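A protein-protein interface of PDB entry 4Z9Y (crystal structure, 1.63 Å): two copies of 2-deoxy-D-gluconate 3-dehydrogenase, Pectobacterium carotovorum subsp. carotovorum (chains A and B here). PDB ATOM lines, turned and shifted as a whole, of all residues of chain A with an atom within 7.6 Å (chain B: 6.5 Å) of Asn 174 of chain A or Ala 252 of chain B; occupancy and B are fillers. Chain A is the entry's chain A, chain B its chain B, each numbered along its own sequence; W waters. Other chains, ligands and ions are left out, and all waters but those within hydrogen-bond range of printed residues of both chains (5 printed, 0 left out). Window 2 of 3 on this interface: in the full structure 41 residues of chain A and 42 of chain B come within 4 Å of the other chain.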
ATOM      1  N   MET A 166      38.905 -12.498 -19.333  1.00  0.00           N
ATOM      2  CA  MET A 166      38.246 -13.782 -19.103  1.00  0.00           C
ATOM      3  C   MET A 166      37.648 -13.823 -17.693  1.00  0.00           C
ATOM      4  O   MET A 166      36.541 -14.309 -17.479  1.00  0.00           O
ATOM      5  CB  MET A 166      39.229 -14.940 -19.341  1.00  0.00           C
ATOM      6  CG  MET A 166      38.566 -16.290 -19.470  1.00  0.00           C
ATOM      7  SD  MET A 166      39.626 -17.437 -20.389  1.00  0.00           S
ATOM      8  CE  MET A 166      40.836 -17.698 -19.118  1.00  0.00           C
ATOM      9  N   GLY A 167      38.376 -13.266 -16.730  1.00  0.00           N
ATOM     10  CA  GLY A 167      37.911 -13.230 -15.347  1.00  0.00           C
ATOM     11  C   GLY A 167      36.704 -12.345 -15.144  1.00  0.00           C
ATOM     12  O   GLY A 167      35.717 -12.777 -14.551  1.00  0.00           O
ATOM     13  N   VAL A 168      36.759 -11.111 -15.635  1.00  0.00           N
ATOM     14  CA  VAL A 168      35.643 -10.149 -15.433  1.00  0.00           C
ATOM     15  C   VAL A 168      34.393 -10.579 -16.189  1.00  0.00           C
ATOM     16  O   VAL A 168      33.270 -10.276 -15.789  1.00  0.00           O
ATOM     17  CB  VAL A 168      35.991  -8.679 -15.793  1.00  0.00           C
ATOM     18  CG1 VAL A 168      37.142  -8.178 -14.954  1.00  0.00           C
ATOM     19  CG2 VAL A 168      36.256  -8.491 -17.276  1.00  0.00           C
ATOM     20  N   THR A 169      34.576 -11.310 -17.284  1.00  0.00           N
ATOM     21  CA  THR A 169      33.441 -11.870 -18.005  1.00  0.00           C
ATOM     22  C   THR A 169      32.644 -12.785 -17.071  1.00  0.00           C
ATOM     23  O   THR A 169      31.402 -12.787 -17.082  1.00  0.00           O
ATOM     24  CB  THR A 169      33.933 -12.619 -19.262  1.00  0.00           C
ATOM     25  OG1 THR A 169      34.546 -11.667 -20.136  1.00  0.00           O
ATOM     26  CG2 THR A 169      32.794 -13.308 -20.011  1.00  0.00           C
ATOM     27  N   ARG A 170      33.362 -13.569 -16.279  1.00  0.00           N
ATOM     28  CA  ARG A 170      32.716 -14.449 -15.296  1.00  0.00           C
ATOM     29  C   ARG A 170      31.912 -13.627 -14.287  1.00  0.00           C
ATOM     30  O   ARG A 170      30.730 -13.892 -14.058  1.00  0.00           O
ATOM     31  CB  ARG A 170      33.752 -15.282 -14.549  1.00  0.00           C
ATOM     32  CG  ARG A 170      34.454 -16.345 -15.370  1.00  0.00           C
ATOM     33  CD  ARG A 170      35.491 -17.107 -14.555  1.00  0.00           C
ATOM     34  NE  ARG A 170      36.215 -18.042 -15.416  1.00  0.00           N
ATOM     35  CZ  ARG A 170      37.515 -18.012 -15.673  1.00  0.00           C
ATOM     36  NH1 ARG A 170      38.310 -17.122 -15.100  1.00  0.00           N
ATOM     37  NH2 ARG A 170      38.027 -18.918 -16.506  1.00  0.00           N
ATOM     38  N   LEU A 171      32.552 -12.617 -13.707  1.00  0.00           N
ATOM     39  CA  LEU A 171      31.902 -11.813 -12.657  1.00  0.00           C
ATOM     40  C   LEU A 171      30.693 -11.052 -13.192  1.00  0.00           C
ATOM     41  O   LEU A 171      29.657 -10.970 -12.532  1.00  0.00           O
ATOM     42  CB  LEU A 171      32.905 -10.866 -11.983  1.00  0.00           C
ATOM     43  CG  LEU A 171      32.292  -9.925 -10.926  1.00  0.00           C
ATOM     44  CD1 LEU A 171      33.257  -9.768  -9.759  1.00  0.00           C
ATOM     45  CD2 LEU A 171      31.907  -8.582 -11.538  1.00  0.00           C
ATOM     46  N   MET A 172      30.807 -10.501 -14.395  1.00  0.00           N
ATOM     47  CA  MET A 172      29.701  -9.750 -14.979  1.00  0.00           C
ATOM     48  C   MET A 172      28.489 -10.665 -15.160  1.00  0.00           C
ATOM     49  O   MET A 172      27.362 -10.284 -14.855  1.00  0.00           O
ATOM     50  CB  MET A 172      30.117  -9.135 -16.319  1.00  0.00           C
ATOM     51  CG  MET A 172      31.104  -7.998 -16.239  1.00  0.00           C
ATOM     52  SD  MET A 172      31.655  -7.593 -17.932  1.00  0.00           S
ATOM     53  CE  MET A 172      32.737  -6.213 -17.612  1.00  0.00           C
ATOM     54  N   ALA A 173      28.722 -11.875 -15.655  1.00  0.00           N
ATOM     55  CA  ALA A 173      27.663 -12.873 -15.747  1.00  0.00           C
ATOM     56  C   ALA A 173      27.040 -13.166 -14.388  1.00  0.00           C
ATOM     57  O   ALA A 173      25.822 -13.219 -14.235  1.00  0.00           O
ATOM     58  CB  ALA A 173      28.209 -14.170 -16.320  1.00  0.00           C
ATOM     59  N   ASN A 174      27.896 -13.360 -13.397  1.00  0.00           N
ATOM     60  CA  ASN A 174      27.422 -13.687 -12.059  1.00  0.00           C
ATOM     61  C   ASN A 174      26.432 -12.668 -11.535  1.00  0.00           C
ATOM     62  O   ASN A 174      25.432 -13.030 -10.926  1.00  0.00           O
ATOM     63  CB  ASN A 174      28.582 -13.814 -11.084  1.00  0.00           C
ATOM     64  CG  ASN A 174      29.476 -14.997 -11.390  1.00  0.00           C
ATOM     65  OD1 ASN A 174      29.076 -15.951 -12.066  1.00  0.00           O
ATOM     66  ND2 ASN A 174      30.712 -14.930 -10.908  1.00  0.00           N
ATOM     67  N   GLU A 175      26.713 -11.399 -11.766  1.00  0.00           N
ATOM     68  CA  GLU A 175      25.861 -10.334 -11.237  1.00  0.00           C
ATOM     69  C   GLU A 175      24.666  -9.994 -12.126  1.00  0.00           C
ATOM     70  O   GLU A 175      23.619  -9.556 -11.629  1.00  0.00           O
ATOM     71  CB  GLU A 175      26.686  -9.086 -10.984  1.00  0.00           C
ATOM     72  CG  GLU A 175      27.687  -9.254  -9.852  1.00  0.00           C
ATOM     73  CD  GLU A 175      28.212  -7.941  -9.292  1.00  0.00           C
ATOM     74  OE1 GLU A 175      29.434  -7.831  -9.083  1.00  0.00           O
ATOM     75  OE2 GLU A 175      27.422  -7.021  -9.027  1.00  0.00           O
ATOM     76  N   TRP A 176      24.818 -10.137 -13.440  1.00  0.00           N
ATOM     77  CA  TRP A 176      23.826  -9.605 -14.360  1.00  0.00           C
ATOM     78  C   TRP A 176      22.967 -10.660 -15.068  1.00  0.00           C
ATOM     79  O   TRP A 176      21.990 -10.306 -15.733  1.00  0.00           O
ATOM     80  CB  TRP A 176      24.516  -8.689 -15.381  1.00  0.00           C
ATOM     81  CG  TRP A 176      25.231  -7.539 -14.753  1.00  0.00           C
ATOM     82  CD1 TRP A 176      24.979  -6.982 -13.527  1.00  0.00           C
ATOM     83  CD2 TRP A 176      26.291  -6.775 -15.323  1.00  0.00           C
ATOM     84  NE1 TRP A 176      25.828  -5.935 -13.296  1.00  0.00           N
ATOM     85  CE2 TRP A 176      26.647  -5.786 -14.382  1.00  0.00           C
ATOM     86  CE3 TRP A 176      27.003  -6.847 -16.529  1.00  0.00           C
ATOM     87  CZ2 TRP A 176      27.677  -4.872 -14.612  1.00  0.00           C
ATOM     88  CZ3 TRP A 176      28.014  -5.939 -16.752  1.00  0.00           C
ATOM     89  CH2 TRP A 176      28.336  -4.960 -15.803  1.00  0.00           C
ATOM     90  N   ALA A 177      23.314 -11.942 -14.941  1.00  0.00           N
ATOM     91  CA  ALA A 177      22.551 -13.020 -15.580  1.00  0.00           C
ATOM     92  C   ALA A 177      21.098 -12.998 -15.133  1.00  0.00           C
ATOM     93  O   ALA A 177      20.201 -13.294 -15.916  1.00  0.00           O
ATOM     94  CB  ALA A 177      23.172 -14.382 -15.292  1.00  0.00           C
ATOM     95  N   LYS A 178      20.869 -12.624 -13.883  1.00  0.00           N
ATOM     96  CA  LYS A 178      19.496 -12.559 -13.359  1.00  0.00           C
ATOM     97  C   LYS A 178      18.625 -11.537 -14.087  1.00  0.00           C
ATOM     98  O   LYS A 178      17.405 -11.624 -14.024  1.00  0.00           O
ATOM     99  CB  LYS A 178      19.498 -12.253 -11.865  1.00  0.00           C
ATOM    100  CG  LYS A 178      19.918 -10.844 -11.538  1.00  0.00           C
ATOM    101  CD  LYS A 178      19.977 -10.620 -10.044  1.00  0.00           C
ATOM    102  CE  LYS A 178      19.963  -9.136  -9.760  1.00  0.00           C
ATOM    103  NZ  LYS A 178      19.977  -8.869  -8.302  1.00  0.00           N
ATOM    104  N   ILE A 181      20.837 -10.824 -18.912  1.00  0.00           N
ATOM    105  CA  ILE A 181      22.026 -10.324 -19.594  1.00  0.00           C
ATOM    106  C   ILE A 181      23.038 -11.458 -19.678  1.00  0.00           C
ATOM    107  O   ILE A 181      23.371 -12.074 -18.658  1.00  0.00           O
ATOM    108  CB  ILE A 181      22.630  -9.102 -18.870  1.00  0.00           C
ATOM    109  CG1 ILE A 181      21.632  -7.941 -18.865  1.00  0.00           C
ATOM    110  CG2 ILE A 181      23.925  -8.674 -19.536  1.00  0.00           C
ATOM    111  CD1 ILE A 181      22.015  -6.789 -17.981  1.00  0.00           C
ATOM    112  N   VAL A 183      26.839 -12.331 -20.613  1.00  0.00           N
ATOM    113  CA  VAL A 183      28.163 -11.771 -20.804  1.00  0.00           C
ATOM    114  C   VAL A 183      29.081 -12.949 -21.075  1.00  0.00           C
ATOM    115  O   VAL A 183      29.272 -13.800 -20.208  1.00  0.00           O
ATOM    116  CB  VAL A 183      28.637 -10.995 -19.572  1.00  0.00           C
ATOM    117  CG1 VAL A 183      29.937 -10.268 -19.889  1.00  0.00           C
ATOM    118  CG2 VAL A 183      27.563 -10.021 -19.116  1.00  0.00           C
ATOM    119  N   ASN A 240      26.603 -18.399 -20.261  1.00  0.00           N
ATOM    120  CA  ASN A 240      26.871 -17.164 -19.546  1.00  0.00           C
ATOM    121  C   ASN A 240      28.173 -17.226 -18.764  1.00  0.00           C
ATOM    122  O   ASN A 240      28.488 -18.236 -18.120  1.00  0.00           O
ATOM    123  CB  ASN A 240      25.689 -16.829 -18.627  1.00  0.00           C
ATOM    124  CG  ASN A 240      25.340 -15.353 -18.636  1.00  0.00           C
ATOM    125  OD1 ASN A 240      26.200 -14.496 -18.818  1.00  0.00           O
ATOM    126  ND2 ASN A 240      24.078 -15.054 -18.407  1.00  0.00           N
ATOM    127  N   GLY A 241      28.949 -16.155 -18.872  1.00  0.00           N
ATOM    128  CA  GLY A 241      30.240 -16.041 -18.230  1.00  0.00           C
ATOM    129  C   GLY A 241      31.357 -16.856 -18.833  1.00  0.00           C
ATOM    130  O   GLY A 241      32.397 -17.049 -18.206  1.00  0.00           O
ATOM    131  N   TYR A 242      31.161 -17.294 -20.065  1.00  0.00           N
ATOM    132  CA  TYR A 242      32.044 -18.292 -20.659  1.00  0.00           C
ATOM    133  C   TYR A 242      32.824 -17.746 -21.847  1.00  0.00           C
ATOM    134  O   TYR A 242      32.336 -16.900 -22.590  1.00  0.00           O
ATOM    135  CB  TYR A 242      31.233 -19.518 -21.054  1.00  0.00           C
ATOM    136  CG  TYR A 242      32.062 -20.778 -21.151  1.00  0.00           C
ATOM    137  CD1 TYR A 242      32.470 -21.469 -20.012  1.00  0.00           C
ATOM    138  CD2 TYR A 242      32.437 -21.269 -22.385  1.00  0.00           C
ATOM    139  CE1 TYR A 242      33.263 -22.621 -20.125  1.00  0.00           C
ATOM    140  CE2 TYR A 242      33.207 -22.398 -22.504  1.00  0.00           C
ATOM    141  CZ  TYR A 242      33.616 -23.068 -21.390  1.00  0.00           C
ATOM    142  OH  TYR A 242      34.359 -24.218 -21.584  1.00  0.00           O
ATOM    143  N   ARG B 212      23.384 -20.782  -6.706  1.00  0.00           N
ATOM    144  CA  ARG B 212      24.723 -20.725  -7.290  1.00  0.00           C
ATOM    145  C   ARG B 212      24.724 -20.806  -8.816  1.00  0.00           C
ATOM    146  O   ARG B 212      25.787 -20.866  -9.423  1.00  0.00           O
ATOM    147  CB  ARG B 212      25.578 -21.854  -6.725  1.00  0.00           C
ATOM    148  CG  ARG B 212      25.766 -21.770  -5.214  1.00  0.00           C
ATOM    149  CD  ARG B 212      26.232 -23.106  -4.658  1.00  0.00           C
ATOM    150  NE  ARG B 212      27.498 -23.516  -5.263  1.00  0.00           N
ATOM    151  CZ  ARG B 212      28.002 -24.747  -5.230  1.00  0.00           C
ATOM    152  NH1 ARG B 212      27.362 -25.738  -4.615  1.00  0.00           N
ATOM    153  NH2 ARG B 212      29.163 -24.990  -5.828  1.00  0.00           N
ATOM    154  N   PRO B 214      23.990 -18.385 -11.733  1.00  0.00           N
ATOM    155  CA  PRO B 214      23.660 -16.991 -12.025  1.00  0.00           C
ATOM    156  C   PRO B 214      22.344 -16.771 -12.769  1.00  0.00           C
ATOM    157  O   PRO B 214      21.615 -15.848 -12.430  1.00  0.00           O
ATOM    158  CB  PRO B 214      24.864 -16.523 -12.854  1.00  0.00           C
ATOM    159  CG  PRO B 214      25.993 -17.309 -12.274  1.00  0.00           C
ATOM    160  CD  PRO B 214      25.419 -18.661 -11.984  1.00  0.00           C
ATOM    161  N   ALA B 215      22.035 -17.616 -13.750  1.00  0.00           N
ATOM    162  CA  ALA B 215      20.778 -17.506 -14.499  1.00  0.00           C
ATOM    163  C   ALA B 215      19.528 -17.678 -13.614  1.00  0.00           C
ATOM    164  O   ALA B 215      18.429 -17.254 -13.987  1.00  0.00           O
ATOM    165  CB  ALA B 215      20.761 -18.513 -15.642  1.00  0.00           C
ATOM    166  N   ASP B 247      25.481 -23.649 -19.153  1.00  0.00           N
ATOM    167  CA  ASP B 247      25.344 -23.890 -17.725  1.00  0.00           C
ATOM    168  C   ASP B 247      24.756 -22.757 -16.904  1.00  0.00           C
ATOM    169  O   ASP B 247      24.803 -22.814 -15.686  1.00  0.00           O
ATOM    170  CB  ASP B 247      26.712 -24.253 -17.143  1.00  0.00           C
ATOM    171  CG  ASP B 247      27.678 -23.074 -17.138  1.00  0.00           C
ATOM    172  OD1 ASP B 247      27.334 -22.010 -17.712  1.00  0.00           O
ATOM    173  OD2 ASP B 247      28.779 -23.221 -16.564  1.00  0.00           O
ATOM    174  N   GLY B 249      25.856 -19.993 -16.209  1.00  0.00           N
ATOM    175  CA  GLY B 249      26.871 -19.353 -15.393  1.00  0.00           C
ATOM    176  C   GLY B 249      27.460 -20.180 -14.275  1.00  0.00           C
ATOM    177  O   GLY B 249      28.228 -19.648 -13.486  1.00  0.00           O
ATOM    178  N   TRP B 250      27.092 -21.459 -14.173  1.00  0.00           N
ATOM    179  CA  TRP B 250      27.567 -22.315 -13.080  1.00  0.00           C
ATOM    180  C   TRP B 250      29.077 -22.211 -12.875  1.00  0.00           C
ATOM    181  O   TRP B 250      29.538 -21.963 -11.773  1.00  0.00           O
ATOM    182  CB  TRP B 250      27.170 -23.779 -13.291  1.00  0.00           C
ATOM    183  CG  TRP B 250      27.694 -24.652 -12.194  1.00  0.00           C
ATOM    184  CD1 TRP B 250      28.837 -25.387 -12.211  1.00  0.00           C
ATOM    185  CD2 TRP B 250      27.121 -24.828 -10.886  1.00  0.00           C
ATOM    186  NE1 TRP B 250      29.005 -26.035 -11.004  1.00  0.00           N
ATOM    187  CE2 TRP B 250      27.960 -25.714 -10.181  1.00  0.00           C
ATOM    188  CE3 TRP B 250      25.966 -24.349 -10.258  1.00  0.00           C
ATOM    189  CZ2 TRP B 250      27.686 -26.120  -8.868  1.00  0.00           C
ATOM    190  CZ3 TRP B 250      25.702 -24.753  -8.956  1.00  0.00           C
ATOM    191  CH2 TRP B 250      26.562 -25.622  -8.277  1.00  0.00           C
ATOM    192  N   LEU B 251      29.842 -22.402 -13.947  1.00  0.00           N
ATOM    193  CA  LEU B 251      31.303 -22.384 -13.851  1.00  0.00           C
ATOM    194  C   LEU B 251      31.854 -20.990 -13.548  1.00  0.00           C
ATOM    195  O   LEU B 251      32.940 -20.861 -12.984  1.00  0.00           O
ATOM    196  CB  LEU B 251      31.927 -22.942 -15.127  1.00  0.00           C
ATOM    197  CG  LEU B 251      31.736 -24.443 -15.376  1.00  0.00           C
ATOM    198  CD1 LEU B 251      32.295 -24.788 -16.742  1.00  0.00           C
ATOM    199  CD2 LEU B 251      32.365 -25.306 -14.289  1.00  0.00           C
ATOM    200  N   ALA B 252      31.113 -19.952 -13.919  1.00  0.00           N
ATOM    201  CA  ALA B 252      31.566 -18.585 -13.686  1.00  0.00           C
ATOM    202  C   ALA B 252      31.501 -18.178 -12.221  1.00  0.00           C
ATOM    203  O   ALA B 252      32.242 -17.314 -11.787  1.00  0.00           O
ATOM    204  CB  ALA B 252      30.748 -17.605 -14.507  1.00  0.00           C
ATOM    205  N   ARG B 253      30.606 -18.782 -11.453  1.00  0.00           N
ATOM    206  CA  ARG B 253      30.285 -18.255 -10.126  1.00  0.00           C
ATOM    207  C   ARG B 253      31.425 -18.424  -9.122  1.00  0.00           C
ATOM    208  O   ARG B 253      32.069 -19.462  -9.122  1.00  0.00           O
ATOM    209  CB  ARG B 253      29.002 -18.902  -9.617  1.00  0.00           C
ATOM    210  CG  ARG B 253      28.471 -18.330  -8.318  1.00  0.00           C
ATOM    211  CD  ARG B 253      28.230 -16.838  -8.389  1.00  0.00           C
ATOM    212  NE  ARG B 253      27.887 -16.310  -7.069  1.00  0.00           N
ATOM    213  CZ  ARG B 253      28.765 -15.958  -6.129  1.00  0.00           C
ATOM    214  NH1 ARG B 253      30.085 -16.056  -6.331  1.00  0.00           N
ATOM    215  NH2 ARG B 253      28.314 -15.488  -4.967  1.00  0.00           N
HETATM  216  O   HOH W   1      29.825 -20.447 -16.872  1.00  0.00           O
HETATM  217  O   HOH W   2      28.074 -20.848 -19.987  1.00  0.00           O
HETATM  218  O   HOH W   3      16.608 -15.025 -13.834  1.00  0.00           O
HETATM  219  O   HOH W   4      32.529 -19.561 -16.846  1.00  0.00           O
HETATM  220  O   HOH W   5      22.775 -13.147 -11.754  1.00  0.00           O
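ND2 of Asn 174 of chain A is in hydrogen-bond range of O of Ala 252 of chain B, 3.0 Å away. The side-chain amide oxygen (OD1) of Asn 174 of chain A lies close to the backbone NH (N) of Arg 253 of chain B (3.3 Å).
The backbone carbonyl oxygen (O) of Arg 170 of chain A lies close to the side-chain amide oxygen (OD1) of Asn 174 of chain A, at 3.3 Å. O of Ile 181 of chain A lies within hydrogen-bond range of ND2 of Asn 240 of chain A (3.1 Å). The backbone NH (N) of Val 183 of chain A lies within hydrogen-bond range of the side-chain amide oxygen (OD1) of Asn 240 of chain A, 2.9 Å away. The backbone NH of Gly 249 of chain B is in hydrogen-bond range of the side-chain carboxylate of Asp 247 of chain B, at 2.9 Å. OD2 of Asp 247 of chain B lies within hydrogen-bond range of N of Trp 250 of chain B (3.4 Å). OD2 of Asp 247 of chain B lies within hydrogen-bond range of N of Leu 251 of chain B (2.9 Å).
Ala 252 of chain B touches Arg 170 of chain A (CB to O, 3.7 Å). Ala 173 of chain A touches Pro 214 of chain B (O to CB, 3.7 Å). Asn 174 of chain A touches Pro 214 of chain B (OD1 to CG, 3.4 Å). Ala 177 of chain A touches Pro 214 of chain B (CB to C, 3.6 Å). Ala 177 of chain A touches Ala 215 of chain B (CB to N, 3.8 Å). Pro 214 of chain B touches Lys 178 of chain A. Asn 240 of chain A touches Asp 247 of chain B. CA of Gly 249 of chain B touches O of Asn 240 of chain A, 3.4 Å away.
Met 172 of chain A touches none of the printed residues of chain B. Of chain B, only Pro 214 (3.4 Å), Ala 252 (3.0 Å) and Arg 253 (3.2 Å) come within 4 Å of Asn 174 of chain A. Glu 175 of chain A touches none of the printed residues of chain B. Printed residues of chain B within 4 Å of Ala 177 of chain A: Pro 214 and Ala 215. Of the printed residues of chain B, Asn 240 of chain A touches Asp 247 (3.97 Å) and Gly 249 (3.4 Å). Of the printed residues of chain A, Pro 214 of chain B touches Ala 173, Asn 174, Ala 177 and Lys 178. Printed residues of chain A within 4 Å of Ala 215 of chain B: Ala 177. Ala 252 of chain B touches just these residues of chain A: Arg 170 and Asn 174. Of the printed residues of chain A, Arg 253 of chain B touches Asn 174. The nearest printed residue of chain B that does not touch Ala 173 of chain A is Ala 252 of chain B (4.6 Å).
Of the 18 printed residues of chain A, 6 touch a printed residue of chain B.
No position is printed for both chains.
Water W2 bridges OD1 of Asp 247 of chain B (2.7 Å) and N of Asn 240 of chain A (2.9 Å). Water W5 lies within hydrogen-bond range of the backbone carbonyl oxygen (O) of Asn 174 of chain A (2.8 Å), the backbone NH (N) of Lys 178 of chain A (2.9 Å), the backbone carbonyl oxygen (O) of Pro 214 of chain B (3.0 Å) and the backbone NH (N) of Ala 177 of chain A (3.4 Å). Water W4 lies within hydrogen-bond range of the backbone carbonyl oxygen of Gly 241 of chain A (2.9 Å) and the backbone NH of Ala 252 of chain B (3.3 Å). Water W1 lies within hydrogen-bond range of O of Asn 240 of chain A, OD2 of Asp 247 of chain B and N of Ala 252 of chain B. Water W3 bridges the backbone carbonyl oxygen of Ala 215 of chain B (2.9 Å) and the backbone carbonyl oxygen of Lys 178 of chain A (3.5 Å).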
